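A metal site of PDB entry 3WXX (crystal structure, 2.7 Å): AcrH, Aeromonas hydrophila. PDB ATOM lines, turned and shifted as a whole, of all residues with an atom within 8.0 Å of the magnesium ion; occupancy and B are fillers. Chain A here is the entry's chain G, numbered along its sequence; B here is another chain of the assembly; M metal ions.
The backbone NH (N) of Gly 13 lies within hydrogen-bond range of the backbone carbonyl oxygen (O) of Phe 8.
The side-chain hydroxyl (OH) of Tyr 58 lies close to a ring nitrogen (NE2) of His 57 (3.2 Å).
The backbone carbonyl oxygen of Gly 12 lies within hydrogen-bond range of the side-chain amide nitrogen of Asn 97 of chain B, at 3.1 Å.
OH of Tyr 85 sits at hydrogen-bond distance from O of His 57 (2.5 Å).
The backbone carbonyl oxygen of Gln 10 is in hydrogen-bond range of the backbone NH of Gly 140 of chain B, 3.1 Å away.
N of Gly 140 of chain B lies within hydrogen-bond range of SD of Met 101 of chain B, at 3.5 Å.
The magnesium ion is bound by the backbone carbonyl oxygen (O) of Leu 9 (2.3 Å).
O of Gly 13 is bound to the magnesium ion (2.3 Å).
OH of Tyr 58 binds the magnesium ion (2.3 Å).
Gly 12 touches the magnesium ion (C to MG, 3.2 Å).
CE1 of His 57 touches the magnesium ion, 3.3 Å away.
O of Gly 140 of chain B touches the magnesium ion (3.6 Å).
Six residues have an atom within 4 Å of the magnesium ion: Leu 9, Gly 12, Gly 13, His 57, Tyr 58 and Gly 140 of chain B.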
ATOM      1  N   ILE A   5      20.700   9.015 -19.695  1.00  0.00           N
ATOM      2  CA  ILE A   5      19.858  10.122 -19.268  1.00  0.00           C
ATOM      3  C   ILE A   5      19.769  10.168 -17.754  1.00  0.00           C
ATOM      4  O   ILE A   5      19.947  11.217 -17.194  1.00  0.00           O
ATOM      5  CB  ILE A   5      18.430  10.042 -19.819  1.00  0.00           C
ATOM      6  CG1 ILE A   5      18.400   9.978 -21.346  1.00  0.00           C
ATOM      7  CG2 ILE A   5      17.651  11.262 -19.352  1.00  0.00           C
ATOM      8  CD1 ILE A   5      19.058  11.165 -22.021  1.00  0.00           C
ATOM      9  N   GLU A   6      19.519   9.029 -17.118  1.00  0.00           N
ATOM     10  CA  GLU A   6      19.534   8.919 -15.655  1.00  0.00           C
ATOM     11  C   GLU A   6      20.834   9.390 -15.036  1.00  0.00           C
ATOM     12  O   GLU A   6      20.823  10.215 -14.104  1.00  0.00           O
ATOM     13  CB  GLU A   6      19.271   7.494 -15.225  1.00  0.00           C
ATOM     14  CG  GLU A   6      19.535   7.261 -13.754  1.00  0.00           C
ATOM     15  CD  GLU A   6      19.060   5.918 -13.241  1.00  0.00           C
ATOM     16  OE1 GLU A   6      18.769   5.003 -14.063  1.00  0.00           O
ATOM     17  OE2 GLU A   6      19.030   5.780 -11.996  1.00  0.00           O
ATOM     18  N   ALA A   7      21.958   8.912 -15.535  1.00  0.00           N
ATOM     19  CA  ALA A   7      23.280   9.382 -15.036  1.00  0.00           C
ATOM     20  C   ALA A   7      23.472  10.913 -15.233  1.00  0.00           C
ATOM     21  O   ALA A   7      24.135  11.584 -14.425  1.00  0.00           O
ATOM     22  CB  ALA A   7      24.391   8.656 -15.745  1.00  0.00           C
ATOM     23  N   PHE A   8      22.889  11.459 -16.290  1.00  0.00           N
ATOM     24  CA  PHE A   8      22.930  12.878 -16.520  1.00  0.00           C
ATOM     25  C   PHE A   8      22.137  13.588 -15.414  1.00  0.00           C
ATOM     26  O   PHE A   8      22.599  14.559 -14.812  1.00  0.00           O
ATOM     27  CB  PHE A   8      22.317  13.171 -17.893  1.00  0.00           C
ATOM     28  CG  PHE A   8      22.402  14.606 -18.278  1.00  0.00           C
ATOM     29  CD1 PHE A   8      23.629  15.194 -18.524  1.00  0.00           C
ATOM     30  CD2 PHE A   8      21.238  15.374 -18.372  1.00  0.00           C
ATOM     31  CE1 PHE A   8      23.712  16.540 -18.863  1.00  0.00           C
ATOM     32  CE2 PHE A   8      21.307  16.712 -18.735  1.00  0.00           C
ATOM     33  CZ  PHE A   8      22.547  17.285 -18.992  1.00  0.00           C
ATOM     34  N   LEU A   9      20.943  13.071 -15.192  1.00  0.00           N
ATOM     35  CA  LEU A   9      19.988  13.685 -14.293  1.00  0.00           C
ATOM     36  C   LEU A   9      20.564  13.668 -12.909  1.00  0.00           C
ATOM     37  O   LEU A   9      20.458  14.658 -12.158  1.00  0.00           O
ATOM     38  CB  LEU A   9      18.660  12.928 -14.350  1.00  0.00           C
ATOM     39  CG  LEU A   9      17.503  13.496 -13.542  1.00  0.00           C
ATOM     40  CD1 LEU A   9      17.069  14.823 -14.101  1.00  0.00           C
ATOM     41  CD2 LEU A   9      16.321  12.558 -13.566  1.00  0.00           C
ATOM     42  N   GLN A  10      21.164  12.530 -12.599  1.00  0.00           N
ATOM     43  CA  GLN A  10      21.772  12.264 -11.315  1.00  0.00           C
ATOM     44  C   GLN A  10      22.975  13.162 -11.008  1.00  0.00           C
ATOM     45  O   GLN A  10      23.166  13.578  -9.877  1.00  0.00           O
ATOM     46  CB  GLN A  10      22.231  10.817 -11.236  1.00  0.00           C
ATOM     47  CG  GLN A  10      22.722  10.476  -9.839  1.00  0.00           C
ATOM     48  CD  GLN A  10      22.916   8.999  -9.612  1.00  0.00           C
ATOM     49  OE1 GLN A  10      22.169   8.372  -8.834  1.00  0.00           O
ATOM     50  NE2 GLN A  10      23.902   8.416 -10.295  1.00  0.00           N
ATOM     51  N   ASP A  11      23.789  13.426 -12.013  1.00  0.00           N
ATOM     52  CA  ASP A  11      24.981  14.228 -11.837  1.00  0.00           C
ATOM     53  C   ASP A  11      24.619  15.706 -11.762  1.00  0.00           C
ATOM     54  O   ASP A  11      25.483  16.531 -11.429  1.00  0.00           O
ATOM     55  CB  ASP A  11      25.969  13.991 -12.994  1.00  0.00           C
ATOM     56  CG  ASP A  11      26.586  12.570 -12.967  1.00  0.00           C
ATOM     57  OD1 ASP A  11      26.526  11.905 -11.921  1.00  0.00           O
ATOM     58  OD2 ASP A  11      27.121  12.140 -13.983  1.00  0.00           O
ATOM     59  N   GLY A  12      23.370  16.042 -12.037  1.00  0.00           N
ATOM     60  CA  GLY A  12      22.911  17.385 -11.826  1.00  0.00           C
ATOM     61  C   GLY A  12      22.508  18.078 -13.086  1.00  0.00           C
ATOM     62  O   GLY A  12      22.342  19.307 -13.094  1.00  0.00           O
ATOM     63  N   GLY A  13      22.404  17.344 -14.175  1.00  0.00           N
ATOM     64  CA  GLY A  13      21.841  17.912 -15.359  1.00  0.00           C
ATOM     65  C   GLY A  13      20.380  18.254 -15.143  1.00  0.00           C
ATOM     66  O   GLY A  13      19.683  17.654 -14.249  1.00  0.00           O
ATOM     67  N   THR A  14      19.924  19.174 -15.992  1.00  0.00           N
ATOM     68  CA  THR A  14      18.600  19.719 -15.996  1.00  0.00           C
ATOM     69  C   THR A  14      17.936  19.615 -17.354  1.00  0.00           C
ATOM     70  O   THR A  14      18.574  19.337 -18.348  1.00  0.00           O
ATOM     71  CB  THR A  14      18.654  21.197 -15.700  1.00  0.00           C
ATOM     72  OG1 THR A  14      18.999  21.882 -16.893  1.00  0.00           O
ATOM     73  CG2 THR A  14      19.676  21.477 -14.635  1.00  0.00           C
ATOM     74  N   LEU A  15      16.629  19.799 -17.367  1.00  0.00           N
ATOM     75  CA  LEU A  15      15.830  19.727 -18.576  1.00  0.00           C
ATOM     76  C   LEU A  15      16.233  20.800 -19.568  1.00  0.00           C
ATOM     77  O   LEU A  15      16.107  20.612 -20.762  1.00  0.00           O
ATOM     78  CB  LEU A  15      14.338  19.870 -18.215  1.00  0.00           C
ATOM     79  CG  LEU A  15      13.300  19.752 -19.337  1.00  0.00           C
ATOM     80  CD1 LEU A  15      13.243  18.351 -19.897  1.00  0.00           C
ATOM     81  CD2 LEU A  15      11.951  20.136 -18.777  1.00  0.00           C
ATOM     82  N   MET A  17      19.282  22.031 -20.120  1.00  0.00           N
ATOM     83  CA  MET A  17      20.449  21.433 -20.756  1.00  0.00           C
ATOM     84  C   MET A  17      20.066  20.386 -21.780  1.00  0.00           C
ATOM     85  O   MET A  17      20.633  20.332 -22.870  1.00  0.00           O
ATOM     86  CB  MET A  17      21.319  20.824 -19.654  1.00  0.00           C
ATOM     87  CG  MET A  17      22.098  21.905 -18.951  1.00  0.00           C
ATOM     88  SD  MET A  17      22.992  21.031 -17.438  1.00  0.00           S
ATOM     89  CE  MET A  17      23.394  22.676 -16.482  1.00  0.00           C
ATOM     90  N   HIS A  57      15.933  22.957 -12.122  1.00  0.00           N
ATOM     91  CA  HIS A  57      15.397  22.668 -10.819  1.00  0.00           C
ATOM     92  C   HIS A  57      16.415  22.872  -9.737  1.00  0.00           C
ATOM     93  O   HIS A  57      16.251  22.386  -8.604  1.00  0.00           O
ATOM     94  CB  HIS A  57      14.772  21.267 -10.782  1.00  0.00           C
ATOM     95  CG  HIS A  57      15.739  20.143 -10.956  1.00  0.00           C
ATOM     96  ND1 HIS A  57      16.049  19.624 -12.188  1.00  0.00           N
ATOM     97  CD2 HIS A  57      16.384  19.358 -10.043  1.00  0.00           C
ATOM     98  CE1 HIS A  57      16.893  18.613 -12.043  1.00  0.00           C
ATOM     99  NE2 HIS A  57      17.111  18.434 -10.755  1.00  0.00           N
ATOM    100  N   TYR A  58      17.461  23.611 -10.088  1.00  0.00           N
ATOM    101  CA  TYR A  58      18.459  24.037  -9.105  1.00  0.00           C
ATOM    102  C   TYR A  58      18.493  25.568  -8.905  1.00  0.00           C
ATOM    103  O   TYR A  58      19.184  26.000  -8.031  1.00  0.00           O
ATOM    104  CB  TYR A  58      19.872  23.465  -9.450  1.00  0.00           C
ATOM    105  CG  TYR A  58      19.965  21.941  -9.546  1.00  0.00           C
ATOM    106  CD1 TYR A  58      20.133  21.110  -8.399  1.00  0.00           C
ATOM    107  CD2 TYR A  58      19.896  21.323 -10.773  1.00  0.00           C
ATOM    108  CE1 TYR A  58      20.209  19.706  -8.497  1.00  0.00           C
ATOM    109  CE2 TYR A  58      19.995  19.949 -10.893  1.00  0.00           C
ATOM    110  CZ  TYR A  58      20.146  19.121  -9.780  1.00  0.00           C
ATOM    111  OH  TYR A  58      20.156  17.757 -10.046  1.00  0.00           O
ATOM    112  N   TYR A  85      12.262  24.467  -0.673  1.00  0.00           N
ATOM    113  CA  TYR A  85      13.192  23.926  -1.655  1.00  0.00           C
ATOM    114  C   TYR A  85      14.157  25.026  -2.080  1.00  0.00           C
ATOM    115  O   TYR A  85      15.323  24.759  -2.248  1.00  0.00           O
ATOM    116  CB  TYR A  85      12.475  23.294  -2.856  1.00  0.00           C
ATOM    117  CG  TYR A  85      13.392  22.673  -3.865  1.00  0.00           C
ATOM    118  CD1 TYR A  85      13.818  21.381  -3.723  1.00  0.00           C
ATOM    119  CD2 TYR A  85      13.832  23.379  -4.967  1.00  0.00           C
ATOM    120  CE1 TYR A  85      14.666  20.769  -4.638  1.00  0.00           C
ATOM    121  CE2 TYR A  85      14.700  22.793  -5.885  1.00  0.00           C
ATOM    122  CZ  TYR A  85      15.125  21.474  -5.717  1.00  0.00           C
ATOM    123  OH  TYR A  85      15.982  20.832  -6.636  1.00  0.00           O
ATOM    124  N   ILE B  94      26.935  22.255 -13.851  1.00  0.00           N
ATOM    125  CA  ILE B  94      26.787  20.910 -13.275  1.00  0.00           C
ATOM    126  C   ILE B  94      27.540  20.777 -11.986  1.00  0.00           C
ATOM    127  O   ILE B  94      27.025  20.233 -11.002  1.00  0.00           O
ATOM    128  CB  ILE B  94      27.180  19.816 -14.286  1.00  0.00           C
ATOM    129  CG1 ILE B  94      26.089  19.756 -15.355  1.00  0.00           C
ATOM    130  CG2 ILE B  94      27.318  18.476 -13.602  1.00  0.00           C
ATOM    131  CD1 ILE B  94      26.343  18.740 -16.405  1.00  0.00           C
ATOM    132  N   ASN B  97      25.564  22.748  -9.310  1.00  0.00           N
ATOM    133  CA  ASN B  97      24.464  21.943  -8.875  1.00  0.00           C
ATOM    134  C   ASN B  97      24.898  20.798  -7.946  1.00  0.00           C
ATOM    135  O   ASN B  97      24.264  20.569  -6.916  1.00  0.00           O
ATOM    136  CB  ASN B  97      23.698  21.446 -10.081  1.00  0.00           C
ATOM    137  CG  ASN B  97      23.132  22.581 -10.910  1.00  0.00           C
ATOM    138  OD1 ASN B  97      23.156  23.740 -10.500  1.00  0.00           O
ATOM    139  ND2 ASN B  97      22.641  22.266 -12.081  1.00  0.00           N
ATOM    140  N   MET B 101      23.819  20.393  -3.843  1.00  0.00           N
ATOM    141  CA  MET B 101      23.301  19.183  -3.222  1.00  0.00           C
ATOM    142  C   MET B 101      24.182  18.774  -2.103  1.00  0.00           C
ATOM    143  O   MET B 101      23.717  18.320  -1.065  1.00  0.00           O
ATOM    144  CB  MET B 101      23.150  18.087  -4.258  1.00  0.00           C
ATOM    145  CG  MET B 101      22.040  18.467  -5.233  1.00  0.00           C
ATOM    146  SD  MET B 101      21.772  16.955  -6.463  1.00  0.00           S
ATOM    147  CE  MET B 101      20.173  16.550  -5.474  1.00  0.00           C
ATOM    148  N   ALA B 138      19.429   9.622  -3.744  1.00  0.00           N
ATOM    149  CA  ALA B 138      19.514   9.558  -5.200  1.00  0.00           C
ATOM    150  C   ALA B 138      20.045  10.807  -5.916  1.00  0.00           C
ATOM    151  O   ALA B 138      19.887  10.963  -7.147  1.00  0.00           O
ATOM    152  CB  ALA B 138      18.148   9.147  -5.768  1.00  0.00           C
ATOM    153  N   THR B 139      20.705  11.673  -5.157  1.00  0.00           N
ATOM    154  CA  THR B 139      21.251  12.964  -5.626  1.00  0.00           C
ATOM    155  C   THR B 139      20.367  13.634  -6.689  1.00  0.00           C
ATOM    156  O   THR B 139      19.195  13.854  -6.428  1.00  0.00           O
ATOM    157  CB  THR B 139      22.728  12.848  -5.995  1.00  0.00           C
ATOM    158  OG1 THR B 139      22.908  11.773  -6.903  1.00  0.00           O
ATOM    159  CG2 THR B 139      23.530  12.509  -4.754  1.00  0.00           C
ATOM    160  N   GLY B 140      20.878  13.911  -7.874  1.00  0.00           N
ATOM    161  CA  GLY B 140      20.135  14.671  -8.858  1.00  0.00           C
ATOM    162  C   GLY B 140      18.776  14.095  -9.237  1.00  0.00           C
ATOM    163  O   GLY B 140      17.865  14.837  -9.655  1.00  0.00           O
ATOM    164  N   VAL B 141      18.610  12.780  -9.112  1.00  0.00           N
ATOM    165  CA  VAL B 141      17.287  12.186  -9.396  1.00  0.00           C
ATOM    166  C   VAL B 141      16.310  12.518  -8.283  1.00  0.00           C
ATOM    167  O   VAL B 141      15.158  12.834  -8.546  1.00  0.00           O
ATOM    168  CB  VAL B 141      17.366  10.657  -9.567  1.00  0.00           C
ATOM    169  CG1 VAL B 141      15.988  10.053  -9.718  1.00  0.00           C
ATOM    170  CG2 VAL B 141      18.181  10.356 -10.793  1.00  0.00           C
ATOM    171  N   GLY B 142      16.775  12.436  -7.051  1.00  0.00           N
ATOM    172  CA  GLY B 142      16.014  12.910  -5.899  1.00  0.00           C
ATOM    173  C   GLY B 142      15.594  14.374  -6.031  1.00  0.00           C
ATOM    174  O   GLY B 142      14.447  14.723  -5.815  1.00  0.00           O
ATOM    175  N   ALA B 143      16.531  15.235  -6.409  1.00  0.00           N
ATOM    176  CA  ALA B 143      16.181  16.604  -6.567  1.00  0.00           C
ATOM    177  C   ALA B 143      15.129  16.761  -7.623  1.00  0.00           C
ATOM    178  O   ALA B 143      14.157  17.496  -7.446  1.00  0.00           O
ATOM    179  CB  ALA B 143      17.404  17.428  -6.958  1.00  0.00           C
ATOM    180  N   ALA B 144      15.351  16.128  -8.756  1.00  0.00           N
ATOM    181  CA  ALA B 144      14.402  16.191  -9.873  1.00  0.00           C
ATOM    182  C   ALA B 144      13.002  15.870  -9.413  1.00  0.00           C
ATOM    183  O   ALA B 144      12.125  16.686  -9.504  1.00  0.00           O
ATOM    184  CB  ALA B 144      14.812  15.223 -10.982  1.00  0.00           C
ATOM    185  N   VAL B 145      12.789  14.667  -8.895  1.00  0.00           N
ATOM    186  CA  VAL B 145      11.444  14.306  -8.537  1.00  0.00           C
ATOM    187  C   VAL B 145      10.914  15.216  -7.436  1.00  0.00           C
ATOM    188  O   VAL B 145       9.718  15.507  -7.392  1.00  0.00           O
ATOM    189  CB  VAL B 145      11.342  12.810  -8.124  1.00  0.00           C
ATOM    190  CG1 VAL B 145      12.086  12.562  -6.846  1.00  0.00           C
ATOM    191  CG2 VAL B 145       9.868  12.378  -8.024  1.00  0.00           C
ATOM    192  N   PHE B 199      12.498  11.690 -18.758  1.00  0.00           N
ATOM    193  CA  PHE B 199      13.867  11.147 -18.694  1.00  0.00           C
ATOM    194  C   PHE B 199      13.729   9.660 -18.800  1.00  0.00           C
ATOM    195  O   PHE B 199      12.640   9.165 -19.101  1.00  0.00           O
ATOM    196  CB  PHE B 199      14.540  11.574 -17.382  1.00  0.00           C
ATOM    197  CG  PHE B 199      14.467  13.063 -17.094  1.00  0.00           C
ATOM    198  CD1 PHE B 199      15.401  13.955 -17.622  1.00  0.00           C
ATOM    199  CD2 PHE B 199      13.458  13.575 -16.294  1.00  0.00           C
ATOM    200  CE1 PHE B 199      15.321  15.322 -17.377  1.00  0.00           C
ATOM    201  CE2 PHE B 199      13.376  14.939 -16.029  1.00  0.00           C
ATOM    202  CZ  PHE B 199      14.306  15.805 -16.572  1.00  0.00           C
HETATM  203 MG    MG M   1      19.694  16.796 -12.105  1.00  0.00          MG
